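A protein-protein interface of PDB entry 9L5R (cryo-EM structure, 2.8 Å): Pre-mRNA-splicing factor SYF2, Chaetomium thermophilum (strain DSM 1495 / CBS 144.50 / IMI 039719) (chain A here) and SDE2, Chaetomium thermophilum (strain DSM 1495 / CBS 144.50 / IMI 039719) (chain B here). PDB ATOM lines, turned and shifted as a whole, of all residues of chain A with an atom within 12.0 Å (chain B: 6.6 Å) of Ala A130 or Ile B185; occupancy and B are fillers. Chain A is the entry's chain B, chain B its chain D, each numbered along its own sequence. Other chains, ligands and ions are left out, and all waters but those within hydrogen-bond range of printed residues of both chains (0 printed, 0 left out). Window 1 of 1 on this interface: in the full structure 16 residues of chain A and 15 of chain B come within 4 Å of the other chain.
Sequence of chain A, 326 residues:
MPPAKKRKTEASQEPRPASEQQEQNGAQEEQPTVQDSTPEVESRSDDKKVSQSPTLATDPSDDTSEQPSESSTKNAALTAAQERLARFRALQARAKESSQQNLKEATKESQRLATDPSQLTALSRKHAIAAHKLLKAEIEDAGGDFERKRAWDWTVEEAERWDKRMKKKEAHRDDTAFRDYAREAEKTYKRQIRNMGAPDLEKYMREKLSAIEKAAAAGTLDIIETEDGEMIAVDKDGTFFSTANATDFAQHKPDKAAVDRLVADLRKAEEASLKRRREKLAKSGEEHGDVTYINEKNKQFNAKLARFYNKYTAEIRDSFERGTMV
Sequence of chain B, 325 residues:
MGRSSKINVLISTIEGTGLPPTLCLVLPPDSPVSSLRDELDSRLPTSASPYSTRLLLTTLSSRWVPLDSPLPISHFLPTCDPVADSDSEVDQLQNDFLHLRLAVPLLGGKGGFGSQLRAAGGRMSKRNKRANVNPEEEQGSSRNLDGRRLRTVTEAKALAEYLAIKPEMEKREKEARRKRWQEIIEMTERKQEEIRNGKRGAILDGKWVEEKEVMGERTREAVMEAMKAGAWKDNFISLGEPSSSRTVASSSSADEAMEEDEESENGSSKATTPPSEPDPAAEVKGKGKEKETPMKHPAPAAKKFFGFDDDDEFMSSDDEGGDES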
ATOM      1  N   LEU A 120      12.847 -23.700  -6.364  1.00  0.00           N
ATOM      2  CA  LEU A 120      12.901 -23.984  -4.932  1.00  0.00           C
ATOM      3  C   LEU A 120      13.119 -22.713  -4.121  1.00  0.00           C
ATOM      4  O   LEU A 120      12.475 -22.516  -3.083  1.00  0.00           O
ATOM      5  CB  LEU A 120      13.991 -25.012  -4.635  1.00  0.00           C
ATOM      6  CG  LEU A 120      13.979 -26.251  -5.531  1.00  0.00           C
ATOM      7  CD1 LEU A 120      15.072 -27.225  -5.114  1.00  0.00           C
ATOM      8  CD2 LEU A 120      12.613 -26.922  -5.527  1.00  0.00           C
ATOM      9  N   THR A 121      14.011 -21.834  -4.582  1.00  0.00           N
ATOM     10  CA  THR A 121      14.187 -20.548  -3.913  1.00  0.00           C
ATOM     11  C   THR A 121      12.927 -19.694  -4.014  1.00  0.00           C
ATOM     12  O   THR A 121      12.564 -18.992  -3.060  1.00  0.00           O
ATOM     13  CB  THR A 121      15.390 -19.808  -4.497  1.00  0.00           C
ATOM     14  OG1 THR A 121      15.291 -19.785  -5.927  1.00  0.00           O
ATOM     15  CG2 THR A 121      16.682 -20.497  -4.093  1.00  0.00           C
ATOM     16  N   ALA A 122      12.236 -19.759  -5.157  1.00  0.00           N
ATOM     17  CA  ALA A 122      10.990 -19.014  -5.314  1.00  0.00           C
ATOM     18  C   ALA A 122       9.913 -19.506  -4.349  1.00  0.00           C
ATOM     19  O   ALA A 122       9.241 -18.699  -3.689  1.00  0.00           O
ATOM     20  CB  ALA A 122      10.510 -19.113  -6.761  1.00  0.00           C
ATOM     21  N   LEU A 123       9.741 -20.827  -4.239  1.00  0.00           N
ATOM     22  CA  LEU A 123       8.739 -21.351  -3.318  1.00  0.00           C
ATOM     23  C   LEU A 123       9.143 -21.115  -1.870  1.00  0.00           C
ATOM     24  O   LEU A 123       8.273 -20.964  -1.007  1.00  0.00           O
ATOM     25  CB  LEU A 123       8.475 -22.837  -3.589  1.00  0.00           C
ATOM     26  CG  LEU A 123       9.524 -23.939  -3.404  1.00  0.00           C
ATOM     27  CD1 LEU A 123       9.516 -24.524  -1.994  1.00  0.00           C
ATOM     28  CD2 LEU A 123       9.318 -25.038  -4.436  1.00  0.00           C
ATOM     29  N   SER A 124      10.449 -21.052  -1.588  1.00  0.00           N
ATOM     30  CA  SER A 124      10.895 -20.612  -0.271  1.00  0.00           C
ATOM     31  C   SER A 124      10.495 -19.169   0.000  1.00  0.00           C
ATOM     32  O   SER A 124      10.124 -18.832   1.130  1.00  0.00           O
ATOM     33  CB  SER A 124      12.409 -20.772  -0.146  1.00  0.00           C
ATOM     34  OG  SER A 124      12.867 -20.272   1.097  1.00  0.00           O
ATOM     35  N   ARG A 125      10.564 -18.308  -1.019  1.00  0.00           N
ATOM     36  CA  ARG A 125      10.120 -16.926  -0.851  1.00  0.00           C
ATOM     37  C   ARG A 125       8.620 -16.843  -0.577  1.00  0.00           C
ATOM     38  O   ARG A 125       8.184 -16.062   0.283  1.00  0.00           O
ATOM     39  CB  ARG A 125      10.490 -16.105  -2.084  1.00  0.00           C
ATOM     40  CG  ARG A 125      11.928 -15.617  -2.080  1.00  0.00           C
ATOM     41  CD  ARG A 125      12.213 -14.731  -3.277  1.00  0.00           C
ATOM     42  NE  ARG A 125      13.644 -14.588  -3.517  1.00  0.00           N
ATOM     43  CZ  ARG A 125      14.171 -13.804  -4.447  1.00  0.00           C
ATOM     44  NH1 ARG A 125      13.412 -13.070  -5.243  1.00  0.00           N
ATOM     45  NH2 ARG A 125      15.494 -13.754  -4.580  1.00  0.00           N
ATOM     46  N   LYS A 126       7.813 -17.633  -1.299  1.00  0.00           N
ATOM     47  CA  LYS A 126       6.378 -17.656  -0.999  1.00  0.00           C
ATOM     48  C   LYS A 126       6.092 -18.220   0.390  1.00  0.00           C
ATOM     49  O   LYS A 126       5.198 -17.723   1.089  1.00  0.00           O
ATOM     50  CB  LYS A 126       5.564 -18.416  -2.050  1.00  0.00           C
ATOM     51  CG  LYS A 126       5.091 -17.563  -3.235  1.00  0.00           C
ATOM     52  CD  LYS A 126       6.125 -17.262  -4.290  1.00  0.00           C
ATOM     53  CE  LYS A 126       6.406 -18.514  -5.096  1.00  0.00           C
ATOM     54  NZ  LYS A 126       7.360 -18.256  -6.200  1.00  0.00           N
ATOM     55  N   HIS A 127       6.839 -19.250   0.807  1.00  0.00           N
ATOM     56  CA  HIS A 127       6.728 -19.749   2.177  1.00  0.00           C
ATOM     57  C   HIS A 127       7.022 -18.657   3.188  1.00  0.00           C
ATOM     58  O   HIS A 127       6.287 -18.501   4.170  1.00  0.00           O
ATOM     59  CB  HIS A 127       7.681 -20.922   2.400  1.00  0.00           C
ATOM     60  CG  HIS A 127       7.608 -21.507   3.780  1.00  0.00           C
ATOM     61  ND1 HIS A 127       8.248 -20.942   4.863  1.00  0.00           N
ATOM     62  CD2 HIS A 127       6.979 -22.607   4.252  1.00  0.00           C
ATOM     63  CE1 HIS A 127       8.007 -21.665   5.942  1.00  0.00           C
ATOM     64  NE2 HIS A 127       7.239 -22.681   5.599  1.00  0.00           N
ATOM     65  N   ALA A 128       8.085 -17.887   2.957  1.00  0.00           N
ATOM     66  CA  ALA A 128       8.477 -16.846   3.898  1.00  0.00           C
ATOM     67  C   ALA A 128       7.414 -15.762   4.002  1.00  0.00           C
ATOM     68  O   ALA A 128       7.030 -15.367   5.109  1.00  0.00           O
ATOM     69  CB  ALA A 128       9.822 -16.249   3.484  1.00  0.00           C
ATOM     70  N   ILE A 129       6.898 -15.292   2.862  1.00  0.00           N
ATOM     71  CA  ILE A 129       5.940 -14.189   2.912  1.00  0.00           C
ATOM     72  C   ILE A 129       4.601 -14.651   3.486  1.00  0.00           C
ATOM     73  O   ILE A 129       3.961 -13.923   4.261  1.00  0.00           O
ATOM     74  CB  ILE A 129       5.787 -13.518   1.532  1.00  0.00           C
ATOM     75  CG1 ILE A 129       5.277 -14.486   0.469  1.00  0.00           C
ATOM     76  CG2 ILE A 129       7.113 -12.930   1.086  1.00  0.00           C
ATOM     77  CD1 ILE A 129       4.922 -13.815  -0.837  1.00  0.00           C
ATOM     78  N   ALA A 130       4.171 -15.876   3.164  1.00  0.00           N
ATOM     79  CA  ALA A 130       2.906 -16.350   3.709  1.00  0.00           C
ATOM     80  C   ALA A 130       3.026 -16.657   5.197  1.00  0.00           C
ATOM     81  O   ALA A 130       2.101 -16.374   5.965  1.00  0.00           O
ATOM     82  CB  ALA A 130       2.421 -17.568   2.931  1.00  0.00           C
ATOM     83  N   ALA A 131       4.166 -17.202   5.632  1.00  0.00           N
ATOM     84  CA  ALA A 131       4.382 -17.422   7.057  1.00  0.00           C
ATOM     85  C   ALA A 131       4.468 -16.102   7.805  1.00  0.00           C
ATOM     86  O   ALA A 131       4.065 -16.012   8.971  1.00  0.00           O
ATOM     87  CB  ALA A 131       5.648 -18.244   7.277  1.00  0.00           C
ATOM     88  N   HIS A 132       4.983 -15.061   7.146  1.00  0.00           N
ATOM     89  CA  HIS A 132       4.997 -13.731   7.736  1.00  0.00           C
ATOM     90  C   HIS A 132       3.576 -13.214   7.937  1.00  0.00           C
ATOM     91  O   HIS A 132       3.249 -12.657   8.997  1.00  0.00           O
ATOM     92  CB  HIS A 132       5.817 -12.791   6.850  1.00  0.00           C
ATOM     93  CG  HIS A 132       5.715 -11.349   7.229  1.00  0.00           C
ATOM     94  ND1 HIS A 132       4.781 -10.497   6.679  1.00  0.00           N
ATOM     95  CD2 HIS A 132       6.443 -10.602   8.091  1.00  0.00           C
ATOM     96  CE1 HIS A 132       4.931  -9.292   7.196  1.00  0.00           C
ATOM     97  NE2 HIS A 132       5.933  -9.328   8.056  1.00  0.00           N
ATOM     98  N   LYS A 133       2.708 -13.422   6.931  1.00  0.00           N
ATOM     99  CA  LYS A 133       1.303 -13.034   7.074  1.00  0.00           C
ATOM    100  C   LYS A 133       0.665 -13.773   8.233  1.00  0.00           C
ATOM    101  O   LYS A 133      -0.043 -13.162   9.042  1.00  0.00           O
ATOM    102  CB  LYS A 133       0.473 -13.353   5.822  1.00  0.00           C
ATOM    103  CG  LYS A 133      -1.004 -12.813   5.859  1.00  0.00           C
ATOM    104  CD  LYS A 133      -2.118 -13.708   6.492  1.00  0.00           C
ATOM    105  CE  LYS A 133      -2.490 -14.949   5.732  1.00  0.00           C
ATOM    106  NZ  LYS A 133      -3.560 -15.717   6.419  1.00  0.00           N
ATOM    107  N   LEU A 134       0.865 -15.094   8.295  1.00  0.00           N
ATOM    108  CA  LEU A 134       0.294 -15.888   9.377  1.00  0.00           C
ATOM    109  C   LEU A 134       0.756 -15.394  10.737  1.00  0.00           C
ATOM    110  O   LEU A 134      -0.084 -15.072  11.578  1.00  0.00           O
ATOM    111  CB  LEU A 134       0.613 -17.376   9.205  1.00  0.00           C
ATOM    112  CG  LEU A 134      -0.309 -18.288   8.381  1.00  0.00           C
ATOM    113  CD1 LEU A 134      -1.664 -18.357   9.068  1.00  0.00           C
ATOM    114  CD2 LEU A 134      -0.502 -17.871   6.943  1.00  0.00           C
ATOM    115  N   LEU A 135       2.070 -15.236  10.924  1.00  0.00           N
ATOM    116  CA  LEU A 135       2.608 -14.820  12.215  1.00  0.00           C
ATOM    117  C   LEU A 135       2.048 -13.475  12.648  1.00  0.00           C
ATOM    118  O   LEU A 135       1.660 -13.302  13.810  1.00  0.00           O
ATOM    119  CB  LEU A 135       4.130 -14.768  12.149  1.00  0.00           C
ATOM    120  CG  LEU A 135       4.811 -14.226  13.398  1.00  0.00           C
ATOM    121  CD1 LEU A 135       4.510 -15.109  14.590  1.00  0.00           C
ATOM    122  CD2 LEU A 135       6.293 -14.140  13.162  1.00  0.00           C
ATOM    123  N   LYS A 136       1.937 -12.532  11.708  1.00  0.00           N
ATOM    124  CA  LYS A 136       1.275 -11.265  12.004  1.00  0.00           C
ATOM    125  C   LYS A 136      -0.183 -11.485  12.401  1.00  0.00           C
ATOM    126  O   LYS A 136      -0.693 -10.839  13.328  1.00  0.00           O
ATOM    127  CB  LYS A 136       1.391 -10.342  10.794  1.00  0.00           C
ATOM    128  CG  LYS A 136       0.693  -9.011  10.920  1.00  0.00           C
ATOM    129  CD  LYS A 136       1.119  -8.097   9.786  1.00  0.00           C
ATOM    130  CE  LYS A 136       0.342  -6.795   9.786  1.00  0.00           C
ATOM    131  NZ  LYS A 136      -1.089  -6.997   9.438  1.00  0.00           N
ATOM    132  N   ALA A 137      -0.864 -12.417  11.724  1.00  0.00           N
ATOM    133  CA  ALA A 137      -2.275 -12.662  12.013  1.00  0.00           C
ATOM    134  C   ALA A 137      -2.481 -13.194  13.427  1.00  0.00           C
ATOM    135  O   ALA A 137      -3.345 -12.693  14.152  1.00  0.00           O
ATOM    136  CB  ALA A 137      -2.874 -13.617  10.984  1.00  0.00           C
ATOM    137  N   GLU A 138      -1.687 -14.183  13.860  1.00  0.00           N
ATOM    138  CA  GLU A 138      -1.855 -14.585  15.260  1.00  0.00           C
ATOM    139  C   GLU A 138      -1.322 -13.562  16.255  1.00  0.00           C
ATOM    140  O   GLU A 138      -1.804 -13.551  17.391  1.00  0.00           O
ATOM    141  CB  GLU A 138      -1.277 -15.962  15.661  1.00  0.00           C
ATOM    142  CG  GLU A 138      -1.934 -17.249  15.097  1.00  0.00           C
ATOM    143  CD  GLU A 138      -1.483 -17.689  13.737  1.00  0.00           C
ATOM    144  OE1 GLU A 138      -0.583 -17.061  13.191  1.00  0.00           O
ATOM    145  OE2 GLU A 138      -2.041 -18.675  13.211  1.00  0.00           O
ATOM    146  N   ILE A 139      -0.382 -12.688  15.883  1.00  0.00           N
ATOM    147  CA  ILE A 139       0.053 -11.677  16.850  1.00  0.00           C
ATOM    148  C   ILE A 139      -1.063 -10.671  17.130  1.00  0.00           C
ATOM    149  O   ILE A 139      -1.424 -10.439  18.291  1.00  0.00           O
ATOM    150  CB  ILE A 139       1.347 -10.990  16.390  1.00  0.00           C
ATOM    151  CG1 ILE A 139       2.520 -11.952  16.538  1.00  0.00           C
ATOM    152  CG2 ILE A 139       1.608  -9.756  17.219  1.00  0.00           C
ATOM    153  CD1 ILE A 139       2.744 -12.403  17.949  1.00  0.00           C
ATOM    154  N   GLU A 140      -1.663 -10.089  16.083  1.00  0.00           N
ATOM    155  CA  GLU A 140      -2.828  -9.255  16.398  1.00  0.00           C
ATOM    156  C   GLU A 140      -4.084 -10.045  16.755  1.00  0.00           C
ATOM    157  O   GLU A 140      -5.053  -9.432  17.218  1.00  0.00           O
ATOM    158  CB  GLU A 140      -3.196  -8.232  15.310  1.00  0.00           C
ATOM    159  CG  GLU A 140      -2.292  -6.992  15.177  1.00  0.00           C
ATOM    160  CD  GLU A 140      -1.090  -7.137  14.286  1.00  0.00           C
ATOM    161  OE1 GLU A 140      -0.940  -8.181  13.646  1.00  0.00           O
ATOM    162  OE2 GLU A 140      -0.298  -6.177  14.214  1.00  0.00           O
ATOM    163  N   ASP A 141      -4.113 -11.364  16.572  1.00  0.00           N
ATOM    164  CA  ASP A 141      -5.244 -12.114  17.106  1.00  0.00           C
ATOM    165  C   ASP A 141      -5.116 -12.318  18.611  1.00  0.00           C
ATOM    166  O   ASP A 141      -6.112 -12.238  19.337  1.00  0.00           O
ATOM    167  CB  ASP A 141      -5.376 -13.451  16.382  1.00  0.00           C
ATOM    168  CG  ASP A 141      -6.288 -13.364  15.177  1.00  0.00           C
ATOM    169  OD1 ASP A 141      -7.132 -12.444  15.142  1.00  0.00           O
ATOM    170  OD2 ASP A 141      -6.166 -14.211  14.268  1.00  0.00           O
ATOM    171  N   PHE A 146       2.365  -6.155  16.743  1.00  0.00           N
ATOM    172  CA  PHE A 146       3.388  -6.744  15.889  1.00  0.00           C
ATOM    173  C   PHE A 146       4.504  -5.750  15.605  1.00  0.00           C
ATOM    174  O   PHE A 146       5.686  -6.117  15.581  1.00  0.00           O
ATOM    175  CB  PHE A 146       2.738  -7.227  14.598  1.00  0.00           C
ATOM    176  CG  PHE A 146       3.683  -7.851  13.627  1.00  0.00           C
ATOM    177  CD1 PHE A 146       4.325  -9.034  13.928  1.00  0.00           C
ATOM    178  CD2 PHE A 146       3.896  -7.275  12.393  1.00  0.00           C
ATOM    179  CE1 PHE A 146       5.184  -9.616  13.021  1.00  0.00           C
ATOM    180  CE2 PHE A 146       4.749  -7.853  11.485  1.00  0.00           C
ATOM    181  CZ  PHE A 146       5.394  -9.024  11.799  1.00  0.00           C
ATOM    182  N   ARG A 150       8.427  -6.042  16.674  1.00  0.00           N
ATOM    183  CA  ARG A 150       9.525  -5.896  15.720  1.00  0.00           C
ATOM    184  C   ARG A 150      10.412  -4.701  16.059  1.00  0.00           C
ATOM    185  O   ARG A 150      11.609  -4.680  15.711  1.00  0.00           O
ATOM    186  CB  ARG A 150       8.952  -5.759  14.316  1.00  0.00           C
ATOM    187  CG  ARG A 150       8.314  -7.017  13.790  1.00  0.00           C
ATOM    188  CD  ARG A 150       8.546  -7.150  12.310  1.00  0.00           C
ATOM    189  NE  ARG A 150       7.846  -6.116  11.562  1.00  0.00           N
ATOM    190  CZ  ARG A 150       7.792  -6.060  10.241  1.00  0.00           C
ATOM    191  NH1 ARG A 150       8.412  -6.948   9.486  1.00  0.00           N
ATOM    192  NH2 ARG A 150       7.096  -5.088   9.662  1.00  0.00           N
ATOM    193  N   ARG B 180      -6.758 -19.924   3.220  1.00  0.00           N
ATOM    194  CA  ARG B 180      -6.134 -19.899   1.903  1.00  0.00           C
ATOM    195  C   ARG B 180      -4.619 -19.831   2.004  1.00  0.00           C
ATOM    196  O   ARG B 180      -3.906 -20.643   1.399  1.00  0.00           O
ATOM    197  CB  ARG B 180      -6.661 -18.716   1.096  1.00  0.00           C
ATOM    198  CG  ARG B 180      -6.333 -18.788  -0.378  1.00  0.00           C
ATOM    199  CD  ARG B 180      -7.279 -17.918  -1.171  1.00  0.00           C
ATOM    200  NE  ARG B 180      -7.085 -16.511  -0.848  1.00  0.00           N
ATOM    201  CZ  ARG B 180      -6.324 -15.682  -1.548  1.00  0.00           C
ATOM    202  NH1 ARG B 180      -5.694 -16.079  -2.643  1.00  0.00           N
ATOM    203  NH2 ARG B 180      -6.188 -14.424  -1.140  1.00  0.00           N
ATOM    204  N   TRP B 181      -4.095 -18.887   2.783  1.00  0.00           N
ATOM    205  CA  TRP B 181      -2.641 -18.826   2.806  1.00  0.00           C
ATOM    206  C   TRP B 181      -2.037 -19.843   3.772  1.00  0.00           C
ATOM    207  O   TRP B 181      -0.852 -20.168   3.636  1.00  0.00           O
ATOM    208  CB  TRP B 181      -2.159 -17.391   3.057  1.00  0.00           C
ATOM    209  CG  TRP B 181      -2.479 -16.496   1.853  1.00  0.00           C
ATOM    210  CD1 TRP B 181      -2.982 -16.910   0.649  1.00  0.00           C
ATOM    211  CD2 TRP B 181      -2.240 -15.083   1.710  1.00  0.00           C
ATOM    212  NE1 TRP B 181      -3.118 -15.848  -0.206  1.00  0.00           N
ATOM    213  CE2 TRP B 181      -2.664 -14.716   0.415  1.00  0.00           C
ATOM    214  CE3 TRP B 181      -1.722 -14.093   2.547  1.00  0.00           C
ATOM    215  CZ2 TRP B 181      -2.590 -13.404  -0.051  1.00  0.00           C
ATOM    216  CZ3 TRP B 181      -1.658 -12.792   2.085  1.00  0.00           C
ATOM    217  CH2 TRP B 181      -2.086 -12.460   0.797  1.00  0.00           C
ATOM    218  N   GLN B 182      -2.842 -20.439   4.661  1.00  0.00           N
ATOM    219  CA  GLN B 182      -2.415 -21.659   5.339  1.00  0.00           C
ATOM    220  C   GLN B 182      -2.231 -22.806   4.354  1.00  0.00           C
ATOM    221  O   GLN B 182      -1.268 -23.574   4.460  1.00  0.00           O
ATOM    222  CB  GLN B 182      -3.432 -22.036   6.416  1.00  0.00           C
ATOM    223  CG  GLN B 182      -3.111 -23.323   7.151  1.00  0.00           C
ATOM    224  CD  GLN B 182      -1.824 -23.243   7.935  1.00  0.00           C
ATOM    225  OE1 GLN B 182      -0.780 -23.709   7.482  1.00  0.00           O
ATOM    226  NE2 GLN B 182      -1.890 -22.660   9.125  1.00  0.00           N
ATOM    227  N   GLU B 183      -3.151 -22.946   3.395  1.00  0.00           N
ATOM    228  CA  GLU B 183      -3.003 -23.971   2.368  1.00  0.00           C
ATOM    229  C   GLU B 183      -1.794 -23.697   1.484  1.00  0.00           C
ATOM    230  O   GLU B 183      -1.101 -24.632   1.067  1.00  0.00           O
ATOM    231  CB  GLU B 183      -4.273 -24.061   1.523  1.00  0.00           C
ATOM    232  CG  GLU B 183      -5.264 -25.114   1.991  1.00  0.00           C
ATOM    233  CD  GLU B 183      -6.411 -25.308   1.020  1.00  0.00           C
ATOM    234  OE1 GLU B 183      -6.355 -24.737  -0.090  1.00  0.00           O
ATOM    235  OE2 GLU B 183      -7.371 -26.029   1.364  1.00  0.00           O
ATOM    236  N   ILE B 184      -1.538 -22.421   1.185  1.00  0.00           N
ATOM    237  CA  ILE B 184      -0.328 -22.052   0.446  1.00  0.00           C
ATOM    238  C   ILE B 184       0.920 -22.464   1.219  1.00  0.00           C
ATOM    239  O   ILE B 184       1.862 -23.039   0.649  1.00  0.00           O
ATOM    240  CB  ILE B 184      -0.326 -20.543   0.132  1.00  0.00           C
ATOM    241  CG1 ILE B 184      -1.526 -20.170  -0.745  1.00  0.00           C
ATOM    242  CG2 ILE B 184       0.985 -20.124  -0.513  1.00  0.00           C
ATOM    243  CD1 ILE B 184      -1.573 -20.900  -2.074  1.00  0.00           C
ATOM    244  N   ILE B 185       0.928 -22.213   2.535  1.00  0.00           N
ATOM    245  CA  ILE B 185       2.024 -22.669   3.389  1.00  0.00           C
ATOM    246  C   ILE B 185       2.187 -24.183   3.291  1.00  0.00           C
ATOM    247  O   ILE B 185       3.268 -24.672   2.956  1.00  0.00           O
ATOM    248  CB  ILE B 185       1.799 -22.213   4.842  1.00  0.00           C
ATOM    249  CG1 ILE B 185       2.143 -20.734   4.994  1.00  0.00           C
ATOM    250  CG2 ILE B 185       2.638 -23.025   5.809  1.00  0.00           C
ATOM    251  CD1 ILE B 185       3.619 -20.455   4.790  1.00  0.00           C
ATOM    252  N   GLU B 186       1.086 -24.925   3.457  1.00  0.00           N
ATOM    253  CA  GLU B 186       1.149 -26.387   3.479  1.00  0.00           C
ATOM    254  C   GLU B 186       1.657 -26.952   2.157  1.00  0.00           C
ATOM    255  O   GLU B 186       2.402 -27.940   2.143  1.00  0.00           O
ATOM    256  CB  GLU B 186      -0.226 -26.965   3.814  1.00  0.00           C
ATOM    257  CG  GLU B 186      -0.646 -26.728   5.252  1.00  0.00           C
ATOM    258  CD  GLU B 186       0.234 -27.463   6.240  1.00  0.00           C
ATOM    259  OE1 GLU B 186       0.659 -28.595   5.931  1.00  0.00           O
ATOM    260  OE2 GLU B 186       0.510 -26.905   7.322  1.00  0.00           O
ATOM    261  N   MET B 187       1.291 -26.317   1.040  1.00  0.00           N
ATOM    262  CA  MET B 187       1.881 -26.678  -0.247  1.00  0.00           C
ATOM    263  C   MET B 187       3.386 -26.428  -0.259  1.00  0.00           C
ATOM    264  O   MET B 187       4.150 -27.233  -0.812  1.00  0.00           O
ATOM    265  CB  MET B 187       1.205 -25.902  -1.375  1.00  0.00           C
ATOM    266  CG  MET B 187      -0.243 -26.268  -1.606  1.00  0.00           C
ATOM    267  SD  MET B 187      -0.985 -25.249  -2.892  1.00  0.00           S
ATOM    268  CE  MET B 187      -0.145 -25.884  -4.335  1.00  0.00           C
ATOM    269  N   THR B 188       3.831 -25.316   0.337  1.00  0.00           N
ATOM    270  CA  THR B 188       5.270 -25.054   0.382  1.00  0.00           C
ATOM    271  C   THR B 188       6.029 -26.092   1.212  1.00  0.00           C
ATOM    272  O   THR B 188       7.088 -26.561   0.782  1.00  0.00           O
ATOM    273  CB  THR B 188       5.553 -23.643   0.893  1.00  0.00           C
ATOM    274  OG1 THR B 188       5.032 -23.506   2.216  1.00  0.00           O
ATOM    275  CG2 THR B 188       4.965 -22.590  -0.031  1.00  0.00           C
ATOM    276  N   GLU B 189       5.517 -26.482   2.390  1.00  0.00           N
ATOM    277  CA  GLU B 189       6.266 -27.541   3.085  1.00  0.00           C
ATOM    278  C   GLU B 189       6.089 -28.915   2.449  1.00  0.00           C
ATOM    279  O   GLU B 189       6.967 -29.762   2.631  1.00  0.00           O
ATOM    280  CB  GLU B 189       6.009 -27.718   4.599  1.00  0.00           C
ATOM    281  CG  GLU B 189       6.463 -26.607   5.557  1.00  0.00           C
ATOM    282  CD  GLU B 189       5.484 -25.496   5.696  1.00  0.00           C
ATOM    283  OE1 GLU B 189       4.414 -25.631   5.105  1.00  0.00           O
ATOM    284  OE2 GLU B 189       5.777 -24.497   6.388  1.00  0.00           O
ATOM    285  N   ARG B 190       5.011 -29.173   1.700  1.00  0.00           N
ATOM    286  CA  ARG B 190       4.970 -30.464   1.020  1.00  0.00           C
ATOM    287  C   ARG B 190       5.972 -30.507  -0.131  1.00  0.00           C
ATOM    288  O   ARG B 190       6.594 -31.549  -0.365  1.00  0.00           O
ATOM    289  CB  ARG B 190       3.548 -30.806   0.550  1.00  0.00           C
ATOM    290  CG  ARG B 190       3.139 -30.320  -0.829  1.00  0.00           C
ATOM    291  CD  ARG B 190       1.646 -30.442  -1.037  1.00  0.00           C
ATOM    292  NE  ARG B 190       1.234 -29.883  -2.318  1.00  0.00           N
ATOM    293  CZ  ARG B 190      -0.026 -29.728  -2.696  1.00  0.00           C
ATOM    294  NH1 ARG B 190      -1.031 -30.068  -1.905  1.00  0.00           N
ATOM    295  NH2 ARG B 190      -0.286 -29.233  -3.901  1.00  0.00           N
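The backbone carbonyl oxygen (O) of Ile B185 sits close to the side-chain carboxylate (OE1) of Glu B189 (2.6 Å).
Of chain B, only Ile B185 (3.6 Å) comes within 4 Å of Ala A130. Ile B185 touches just these residues of chain A: His A127 (3.4 Å), Ala A130 (3.6 Å) and Ala A131 (3.4 Å). No residue of chain A comes within 4 Å of Ile B184. No residue of chain A comes within 4 Å of Glu B186. Met B187 touches none of the printed residues of chain A. Thr B188 touches just these residues of chain A: Leu A123 (3.8 Å) and His A127 (3.0 Å). Of chain A, only His A127 (2.5 Å) comes within 4 Å of Glu B189. Printed residues of chain B within 4 Å of His A127: Ile B185 (3.4 Å), Thr B188 (3.0 Å) and Glu B189 (2.5 Å). Of the printed residues of chain B, Leu A123 touches Thr B188. Phe A146 touches none of the printed residues of chain B. The nearest printed residue of chain B that does not touch Leu A123 is Met B187 (6.1 Å).
Among the printed residues, merely in contact across the chains: His A127 with Thr B188 (3.0 Å), His A127 with Ile B185 (3.4 Å), Lys A133 with Trp B181 (3.4 Å), Ala A131 with Ile B185 (3.4 Å), Ala A130 with Ile B185 (3.6 Å) and Leu A123 with Thr B188 (3.8 Å).
Hydrophobic or aromatic side chains of chain B within 4 Å of the printed part of chain A: Trp B181 and Ile B185. Hydrophobic or aromatic side chains of chain A within 4 Å of the printed part of chain B: His A127, Ala A130 and Ala A131. Along chain A the printed residues that touch a printed residue of chain B span positions 123 to 133. Among the printed residues, 7 pairs touch across the chains. Among the printed residues, no Asp or Glu carboxylate lies within 4 Å of a Lys or Arg side-chain nitrogen of the other chain.
NE2 of His A127 is in hydrogen-bond range of OE2 of Glu B189, at 2.5 Å.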
